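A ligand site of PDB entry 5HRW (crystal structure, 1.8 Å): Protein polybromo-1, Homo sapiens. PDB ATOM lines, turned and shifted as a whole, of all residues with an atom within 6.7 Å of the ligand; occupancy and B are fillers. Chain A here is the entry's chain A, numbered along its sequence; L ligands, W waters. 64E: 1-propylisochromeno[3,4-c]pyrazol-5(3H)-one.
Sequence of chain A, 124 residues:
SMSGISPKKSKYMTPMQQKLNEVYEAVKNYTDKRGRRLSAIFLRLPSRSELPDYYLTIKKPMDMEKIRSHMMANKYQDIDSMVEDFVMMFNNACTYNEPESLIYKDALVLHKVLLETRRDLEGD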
ATOM      1  N   ILE A  41      13.504   8.219   4.059  1.00  0.00           N
ATOM      2  CA  ILE A  41      13.810   7.986   5.492  1.00  0.00           C
ATOM      3  C   ILE A  41      14.700   6.795   5.820  1.00  0.00           C
ATOM      4  O   ILE A  41      15.256   6.725   6.928  1.00  0.00           O
ATOM      5  CB  ILE A  41      12.581   8.046   6.377  1.00  0.00           C
ATOM      6  CG1 ILE A  41      11.718   6.864   6.135  1.00  0.00           C
ATOM      7  CG2 ILE A  41      11.907   9.421   6.127  1.00  0.00           C
ATOM      8  CD1 ILE A  41      12.135   5.626   6.819  1.00  0.00           C
ATOM      9  N   PHE A  42      14.937   5.928   4.836  1.00  0.00           N
ATOM     10  CA  PHE A  42      15.771   4.751   4.959  1.00  0.00           C
ATOM     11  C   PHE A  42      17.277   5.009   4.665  1.00  0.00           C
ATOM     12  O   PHE A  42      18.094   4.104   4.893  1.00  0.00           O
ATOM     13  CB  PHE A  42      15.260   3.649   4.037  1.00  0.00           C
ATOM     14  CG  PHE A  42      13.924   3.109   4.434  1.00  0.00           C
ATOM     15  CD1 PHE A  42      13.831   2.130   5.423  1.00  0.00           C
ATOM     16  CD2 PHE A  42      12.758   3.533   3.813  1.00  0.00           C
ATOM     17  CE1 PHE A  42      12.572   1.651   5.809  1.00  0.00           C
ATOM     18  CE2 PHE A  42      11.498   3.040   4.194  1.00  0.00           C
ATOM     19  CZ  PHE A  42      11.426   2.117   5.194  1.00  0.00           C
ATOM     20  N   LEU A  43      17.609   6.176   4.136  1.00  0.00           N
ATOM     21  CA  LEU A  43      18.981   6.494   3.756  1.00  0.00           C
ATOM     22  C   LEU A  43      19.945   6.427   4.956  1.00  0.00           C
ATOM     23  O   LEU A  43      21.012   5.806   4.827  1.00  0.00           O
ATOM     24  CB  LEU A  43      19.138   7.805   3.048  1.00  0.00           C
ATOM     25  CG  LEU A  43      18.285   8.016   1.779  1.00  0.00           C
ATOM     26  CD1 LEU A  43      18.685   9.361   1.129  1.00  0.00           C
ATOM     27  CD2 LEU A  43      18.311   6.880   0.798  1.00  0.00           C
ATOM     28  N   ARG A  44      19.614   7.079   6.067  1.00  0.00           N
ATOM     29  CA  ARG A  44      20.507   7.177   7.199  1.00  0.00           C
ATOM     30  C   ARG A  44      19.746   7.067   8.526  1.00  0.00           C
ATOM     31  O   ARG A  44      18.879   7.857   8.830  1.00  0.00           O
ATOM     32  CB  ARG A  44      21.309   8.494   7.136  1.00  0.00           C
ATOM     33  CG  ARG A  44      22.469   8.517   8.105  1.00  0.00           C
ATOM     34  CD  ARG A  44      23.600   7.616   7.708  1.00  0.00           C
ATOM     35  NE  ARG A  44      24.647   7.754   8.720  1.00  0.00           N
ATOM     36  CZ  ARG A  44      25.032   6.840   9.627  1.00  0.00           C
ATOM     37  NH1 ARG A  44      24.480   5.638   9.699  1.00  0.00           N
ATOM     38  NH2 ARG A  44      25.986   7.182  10.520  1.00  0.00           N
ATOM     39  N   LEU A  45      20.075   6.059   9.290  1.00  0.00           N
ATOM     40  CA  LEU A  45      19.574   5.909  10.675  1.00  0.00           C
ATOM     41  C   LEU A  45      19.926   7.124  11.538  1.00  0.00           C
ATOM     42  O   LEU A  45      21.108   7.595  11.491  1.00  0.00           O
ATOM     43  CB  LEU A  45      20.120   4.700  11.397  1.00  0.00           C
ATOM     44  CG  LEU A  45      19.387   3.395  11.157  1.00  0.00           C
ATOM     45  CD1 LEU A  45      20.312   2.291  11.627  1.00  0.00           C
ATOM     46  CD2 LEU A  45      18.033   3.386  11.918  1.00  0.00           C
ATOM     47  N   PRO A  46      18.955   7.579  12.346  1.00  0.00           N
ATOM     48  CA  PRO A  46      19.309   8.573  13.367  1.00  0.00           C
ATOM     49  C   PRO A  46      20.250   7.971  14.433  1.00  0.00           C
ATOM     50  O   PRO A  46      20.501   6.731  14.411  1.00  0.00           O
ATOM     51  CB  PRO A  46      17.981   8.990  13.955  1.00  0.00           C
ATOM     52  CG  PRO A  46      16.925   8.572  12.911  1.00  0.00           C
ATOM     53  CD  PRO A  46      17.502   7.265  12.394  1.00  0.00           C
ATOM     54  N   LEU A  51      16.979   7.864  18.373  1.00  0.00           N
ATOM     55  CA  LEU A  51      16.056   6.771  18.135  1.00  0.00           C
ATOM     56  C   LEU A  51      16.443   5.605  19.015  1.00  0.00           C
ATOM     57  O   LEU A  51      16.758   4.495  18.532  1.00  0.00           O
ATOM     58  CB  LEU A  51      16.108   6.407  16.658  1.00  0.00           C
ATOM     59  CG  LEU A  51      14.840   5.663  16.148  1.00  0.00           C
ATOM     60  CD1 LEU A  51      13.593   6.560  16.145  1.00  0.00           C
ATOM     61  CD2 LEU A  51      15.110   5.088  14.776  1.00  0.00           C
ATOM     62  N   TYR A  54      14.836   1.963  18.691  1.00  0.00           N
ATOM     63  CA  TYR A  54      15.262   1.121  17.560  1.00  0.00           C
ATOM     64  C   TYR A  54      16.487   0.300  17.955  1.00  0.00           C
ATOM     65  O   TYR A  54      16.516  -0.895  17.719  1.00  0.00           O
ATOM     66  CB  TYR A  54      15.605   1.970  16.349  1.00  0.00           C
ATOM     67  CG  TYR A  54      16.281   1.245  15.227  1.00  0.00           C
ATOM     68  CD1 TYR A  54      17.664   1.073  15.223  1.00  0.00           C
ATOM     69  CD2 TYR A  54      15.538   0.756  14.146  1.00  0.00           C
ATOM     70  CE1 TYR A  54      18.294   0.437  14.173  1.00  0.00           C
ATOM     71  CE2 TYR A  54      16.174   0.126  13.055  1.00  0.00           C
ATOM     72  CZ  TYR A  54      17.566  -0.042  13.105  1.00  0.00           C
ATOM     73  OH  TYR A  54      18.263  -0.667  12.064  1.00  0.00           O
ATOM     74  N   ILE A  58      16.703  -3.846  17.836  1.00  0.00           N
ATOM     75  CA  ILE A  58      17.269  -4.392  16.579  1.00  0.00           C
ATOM     76  C   ILE A  58      18.731  -4.792  16.819  1.00  0.00           C
ATOM     77  O   ILE A  58      19.551  -3.951  17.181  1.00  0.00           O
ATOM     78  CB  ILE A  58      17.200  -3.296  15.470  1.00  0.00           C
ATOM     79  CG1 ILE A  58      15.756  -2.970  15.087  1.00  0.00           C
ATOM     80  CG2 ILE A  58      18.052  -3.620  14.283  1.00  0.00           C
ATOM     81  CD1 ILE A  58      14.836  -4.133  14.723  1.00  0.00           C
ATOM     82  N   MET A  62      20.817  -1.400  10.117  1.00  0.00           N
ATOM     83  CA  MET A  62      21.115  -1.286   8.698  1.00  0.00           C
ATOM     84  C   MET A  62      20.422  -0.027   8.139  1.00  0.00           C
ATOM     85  O   MET A  62      19.270   0.249   8.475  1.00  0.00           O
ATOM     86  CB  MET A  62      20.544  -2.521   7.987  1.00  0.00           C
ATOM     87  CG  MET A  62      20.964  -2.633   6.524  1.00  0.00           C
ATOM     88  SD  MET A  62      22.744  -2.558   6.148  1.00  0.00           S
ATOM     89  CE  MET A  62      23.171  -4.043   7.002  1.00  0.00           C
ATOM     90  N   ASP A  63      21.070   0.667   7.224  1.00  0.00           N
ATOM     91  CA  ASP A  63      20.468   1.751   6.435  1.00  0.00           C
ATOM     92  C   ASP A  63      21.033   1.727   5.007  1.00  0.00           C
ATOM     93  O   ASP A  63      21.946   0.932   4.740  1.00  0.00           O
ATOM     94  CB  ASP A  63      20.634   3.108   7.149  1.00  0.00           C
ATOM     95  CG  ASP A  63      22.103   3.534   7.403  1.00  0.00           C
ATOM     96  OD1 ASP A  63      23.067   3.091   6.721  1.00  0.00           O
ATOM     97  OD2 ASP A  63      22.240   4.366   8.346  1.00  0.00           O
ATOM     98  N   MET A  64      20.467   2.540   4.108  1.00  0.00           N
ATOM     99  CA  MET A  64      20.876   2.467   2.710  1.00  0.00           C
ATOM    100  C   MET A  64      22.275   3.042   2.523  1.00  0.00           C
ATOM    101  O   MET A  64      22.998   2.557   1.645  1.00  0.00           O
ATOM    102  CB  MET A  64      19.880   3.140   1.801  1.00  0.00           C
ATOM    103  CG  MET A  64      18.575   2.363   1.820  1.00  0.00           C
ATOM    104  SD  MET A  64      17.319   2.871   0.658  1.00  0.00           S
ATOM    105  CE  MET A  64      18.223   2.963  -0.836  1.00  0.00           C
ATOM    106  N   MET A  88      17.091  -7.463   5.403  1.00  0.00           N
ATOM    107  CA  MET A  88      17.281  -7.249   6.862  1.00  0.00           C
ATOM    108  C   MET A  88      16.806  -5.865   7.268  1.00  0.00           C
ATOM    109  O   MET A  88      16.127  -5.731   8.268  1.00  0.00           O
ATOM    110  CB  MET A  88      18.731  -7.404   7.243  1.00  0.00           C
ATOM    111  CG  MET A  88      18.968  -7.352   8.789  1.00  0.00           C
ATOM    112  SD  MET A  88      20.700  -7.724   8.986  1.00  0.00           S
ATOM    113  CE  MET A  88      21.428  -6.208   8.397  1.00  0.00           C
ATOM    114  N   MET A  89      17.148  -4.857   6.467  1.00  0.00           N
ATOM    115  CA  MET A  89      16.687  -3.479   6.706  1.00  0.00           C
ATOM    116  C   MET A  89      15.156  -3.365   6.790  1.00  0.00           C
ATOM    117  O   MET A  89      14.542  -2.790   7.726  1.00  0.00           O
ATOM    118  CB  MET A  89      17.263  -2.526   5.659  1.00  0.00           C
ATOM    119  CG  MET A  89      17.018  -1.040   5.958  1.00  0.00           C
ATOM    120  SD  MET A  89      17.569   0.083   4.681  1.00  0.00           S
ATOM    121  CE  MET A  89      16.279  -0.278   3.454  1.00  0.00           C
ATOM    122  N   PHE A  90      14.460  -3.891   5.797  1.00  0.00           N
ATOM    123  CA  PHE A  90      13.000  -3.874   5.876  1.00  0.00           C
ATOM    124  C   PHE A  90      12.387  -4.750   6.988  1.00  0.00           C
ATOM    125  O   PHE A  90      11.427  -4.329   7.645  1.00  0.00           O
ATOM    126  CB  PHE A  90      12.422  -4.261   4.483  1.00  0.00           C
ATOM    127  CG  PHE A  90      12.857  -3.356   3.389  1.00  0.00           C
ATOM    128  CD1 PHE A  90      12.769  -1.995   3.505  1.00  0.00           C
ATOM    129  CD2 PHE A  90      13.352  -3.912   2.196  1.00  0.00           C
ATOM    130  CE1 PHE A  90      13.199  -1.153   2.471  1.00  0.00           C
ATOM    131  CE2 PHE A  90      13.793  -3.078   1.187  1.00  0.00           C
ATOM    132  CZ  PHE A  90      13.685  -1.710   1.282  1.00  0.00           C
ATOM    133  N   ASN A  91      12.962  -5.918   7.250  1.00  0.00           N
ATOM    134  CA  ASN A  91      12.562  -6.731   8.401  1.00  0.00           C
ATOM    135  C   ASN A  91      12.809  -5.959   9.686  1.00  0.00           C
ATOM    136  O   ASN A  91      11.937  -5.958  10.537  1.00  0.00           O
ATOM    137  CB  ASN A  91      13.287  -8.087   8.446  1.00  0.00           C
ATOM    138  CG  ASN A  91      12.671  -9.073   7.444  1.00  0.00           C
ATOM    139  OD1 ASN A  91      11.470  -9.000   7.136  1.00  0.00           O
ATOM    140  ND2 ASN A  91      13.448  -9.995   6.982  1.00  0.00           N
ATOM    141  N   ASN A  92      13.973  -5.311   9.832  1.00  0.00           N
ATOM    142  CA  ASN A  92      14.181  -4.407  10.985  1.00  0.00           C
ATOM    143  C   ASN A  92      13.064  -3.368  11.136  1.00  0.00           C
ATOM    144  O   ASN A  92      12.464  -3.197  12.244  1.00  0.00           O
ATOM    145  CB  ASN A  92      15.544  -3.687  10.908  1.00  0.00           C
ATOM    146  CG  ASN A  92      16.762  -4.598  11.117  1.00  0.00           C
ATOM    147  OD1 ASN A  92      16.684  -5.734  11.619  1.00  0.00           O
ATOM    148  ND2 ASN A  92      17.939  -4.090  10.718  1.00  0.00           N
ATOM    149  N   ALA A  93      12.765  -2.643  10.069  1.00  0.00           N
ATOM    150  CA  ALA A  93      11.730  -1.583  10.098  1.00  0.00           C
ATOM    151  C   ALA A  93      10.370  -2.139  10.571  1.00  0.00           C
ATOM    152  O   ALA A  93       9.677  -1.507  11.334  1.00  0.00           O
ATOM    153  CB  ALA A  93      11.593  -0.946   8.754  1.00  0.00           C
ATOM    154  N   CYS A  94      10.028  -3.333  10.084  1.00  0.00           N
ATOM    155  CA  CYS A  94       8.771  -3.977  10.407  1.00  0.00           C
ATOM    156  C   CYS A  94       8.787  -4.688  11.783  1.00  0.00           C
ATOM    157  O   CYS A  94       7.747  -5.064  12.266  1.00  0.00           O
ATOM    158  CB  CYS A  94       8.384  -4.947   9.335  1.00  0.00           C
ATOM    159  SG  CYS A  94       7.947  -4.078   7.757  1.00  0.00           S
ATOM    160  N   TYR A  96      10.606  -3.236  14.526  1.00  0.00           N
ATOM    161  CA  TYR A  96      10.602  -2.052  15.403  1.00  0.00           C
ATOM    162  C   TYR A  96       9.281  -1.295  15.312  1.00  0.00           C
ATOM    163  O   TYR A  96       8.731  -0.957  16.335  1.00  0.00           O
ATOM    164  CB  TYR A  96      11.784  -1.140  15.086  1.00  0.00           C
ATOM    165  CG  TYR A  96      11.677   0.207  15.811  1.00  0.00           C
ATOM    166  CD1 TYR A  96      11.517   0.230  17.204  1.00  0.00           C
ATOM    167  CD2 TYR A  96      11.651   1.402  15.131  1.00  0.00           C
ATOM    168  CE1 TYR A  96      11.419   1.425  17.890  1.00  0.00           C
ATOM    169  CE2 TYR A  96      11.525   2.631  15.808  1.00  0.00           C
ATOM    170  CZ  TYR A  96      11.402   2.595  17.199  1.00  0.00           C
ATOM    171  OH  TYR A  96      11.193   3.726  17.885  1.00  0.00           O
ATOM    172  N   ASN A  97       8.760  -1.005  14.118  1.00  0.00           N
ATOM    173  CA  ASN A  97       7.543  -0.252  13.960  1.00  0.00           C
ATOM    174  C   ASN A  97       6.274  -1.093  13.944  1.00  0.00           C
ATOM    175  O   ASN A  97       6.291  -2.297  13.645  1.00  0.00           O
ATOM    176  CB  ASN A  97       7.614   0.583  12.678  1.00  0.00           C
ATOM    177  CG  ASN A  97       8.747   1.605  12.744  1.00  0.00           C
ATOM    178  OD1 ASN A  97       8.582   2.683  13.363  1.00  0.00           O
ATOM    179  ND2 ASN A  97       9.841   1.317  12.077  1.00  0.00           N
ATOM    180  N   ILE A 103       5.996   4.097   7.966  1.00  0.00           N
ATOM    181  CA  ILE A 103       7.279   3.523   7.623  1.00  0.00           C
ATOM    182  C   ILE A 103       7.173   1.980   7.374  1.00  0.00           C
ATOM    183  O   ILE A 103       7.834   1.441   6.487  1.00  0.00           O
ATOM    184  CB  ILE A 103       8.395   3.851   8.663  1.00  0.00           C
ATOM    185  CG1 ILE A 103       9.734   3.314   8.221  1.00  0.00           C
ATOM    186  CG2 ILE A 103       8.132   3.255  10.005  1.00  0.00           C
ATOM    187  CD1 ILE A 103      10.886   3.840   9.057  1.00  0.00           C
HETATM  188  CAG 64E L   1      13.972   3.746  10.778  1.00  0.00           C
HETATM  189  CAD 64E L   1      15.030   3.537   9.888  1.00  0.00           C
HETATM  190  CAC 64E L   1      15.784   4.593   9.345  1.00  0.00           C
HETATM  191  CAB 64E L   1      16.830   4.388   8.421  1.00  0.00           C
HETATM  192  CAA 64E L   1      17.096   3.098   7.995  1.00  0.00           C
HETATM  193  CAF 64E L   1      16.350   2.025   8.498  1.00  0.00           C
HETATM  194  CAE 64E L   1      15.324   2.237   9.447  1.00  0.00           C
HETATM  195  CAJ 64E L   1      14.606   1.130   9.960  1.00  0.00           C
HETATM  196  OAK 64E L   1      14.829  -0.038   9.646  1.00  0.00           O
HETATM  197  OAI 64E L   1      13.576   1.355  10.843  1.00  0.00           O
HETATM  198  CAH 64E L   1      13.266   2.677  11.218  1.00  0.00           C
HETATM  199  NAN 64E L   1      12.324   3.080  12.093  1.00  0.00           N
HETATM  200  NAM 64E L   1      12.377   4.305  12.180  1.00  0.00           N
HETATM  201  CAL 64E L   1      13.372   4.768  11.425  1.00  0.00           C
HETATM  202  CAO 64E L   1      13.667   6.257  11.335  1.00  0.00           C
HETATM  203  CAP 64E L   1      12.672   6.961  12.226  1.00  0.00           C
HETATM  204  CAQ 64E L   1      12.891   8.493  12.172  1.00  0.00           C
HETATM  205  O   HOH W   1      10.065   5.027  13.652  1.00  0.00           O
HETATM  206  O   HOH W   2      17.303  -1.301   9.611  1.00  0.00           O
HETATM  207  O   HOH W   3      16.146   8.006   9.056  1.00  0.00           O
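ND2 of Asn 97 sits close to NAN of the ligand (3.0 Å).
N of Ala 93 lies within hydrogen-bond range of OAK of the ligand (3.4 Å).
The backbone carbonyl oxygen (O) of Ala 93 sits at hydrogen-bond distance from the side-chain amide nitrogen (ND2) of Asn 97 (2.9 Å).
The backbone carbonyl oxygen (O) of Phe 42 is in hydrogen-bond range of the backbone NH (N) of Met 64, at 2.9 Å.
OH of Tyr 54 is in hydrogen-bond range of N of Met 62, at 3.3 Å.
The side-chain carboxylate (OD2) of Asp 63 lies within hydrogen-bond range of the backbone NH (N) of Leu 45, 2.9 Å away.
The guanidinium group (NH1) of Arg 44 is in salt-bridge range of the side-chain carboxylate (OD2) of Asp 63, 2.9 Å away.
The side-chain amide oxygen (OD1) of Asn 92 sits close to the backbone carbonyl oxygen (O) of Met 88, at 3.4 Å.
The backbone carbonyl oxygen of Met 89 sits close to an oxygen (OAK) of the ligand (3.4 Å).
Merely in contact with the ligand: Ile 41 (3.2 Å), Phe 42 (3.4 Å), Met 62 (3.4 Å), Ile 103 (3.4 Å), Tyr 96 (3.5 Å), Tyr 54 (3.6 Å), Leu 45 (3.6 Å), Asp 63 (3.6 Å), Leu 51 (3.8 Å), Asn 92 (3.9 Å) and Arg 44 (3.96 Å).
Hydrophobic or aromatic side chains that line the ligand: Phe 42, Leu 45, Leu 51, Tyr 54, Ala 93, Tyr 96 and Ile 103.
Of the 22 residues printed, 14 come within 4 Å of the ligand.
The nearest printed residue that does not touch the ligand is Pro 46 (4.1 Å).
Water W2 lies within hydrogen-bond range of the side-chain hydroxyl of Tyr 54 (2.7 Å), the backbone carbonyl oxygen of Met 62 (2.7 Å), an oxygen (OAK) of the ligand (2.8 Å) and the side-chain amide nitrogen of Asn 92 (3.1 Å).
Water W1 bridges the side-chain amide oxygen of Asn 97 and a nitrogen (NAM) of the ligand.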
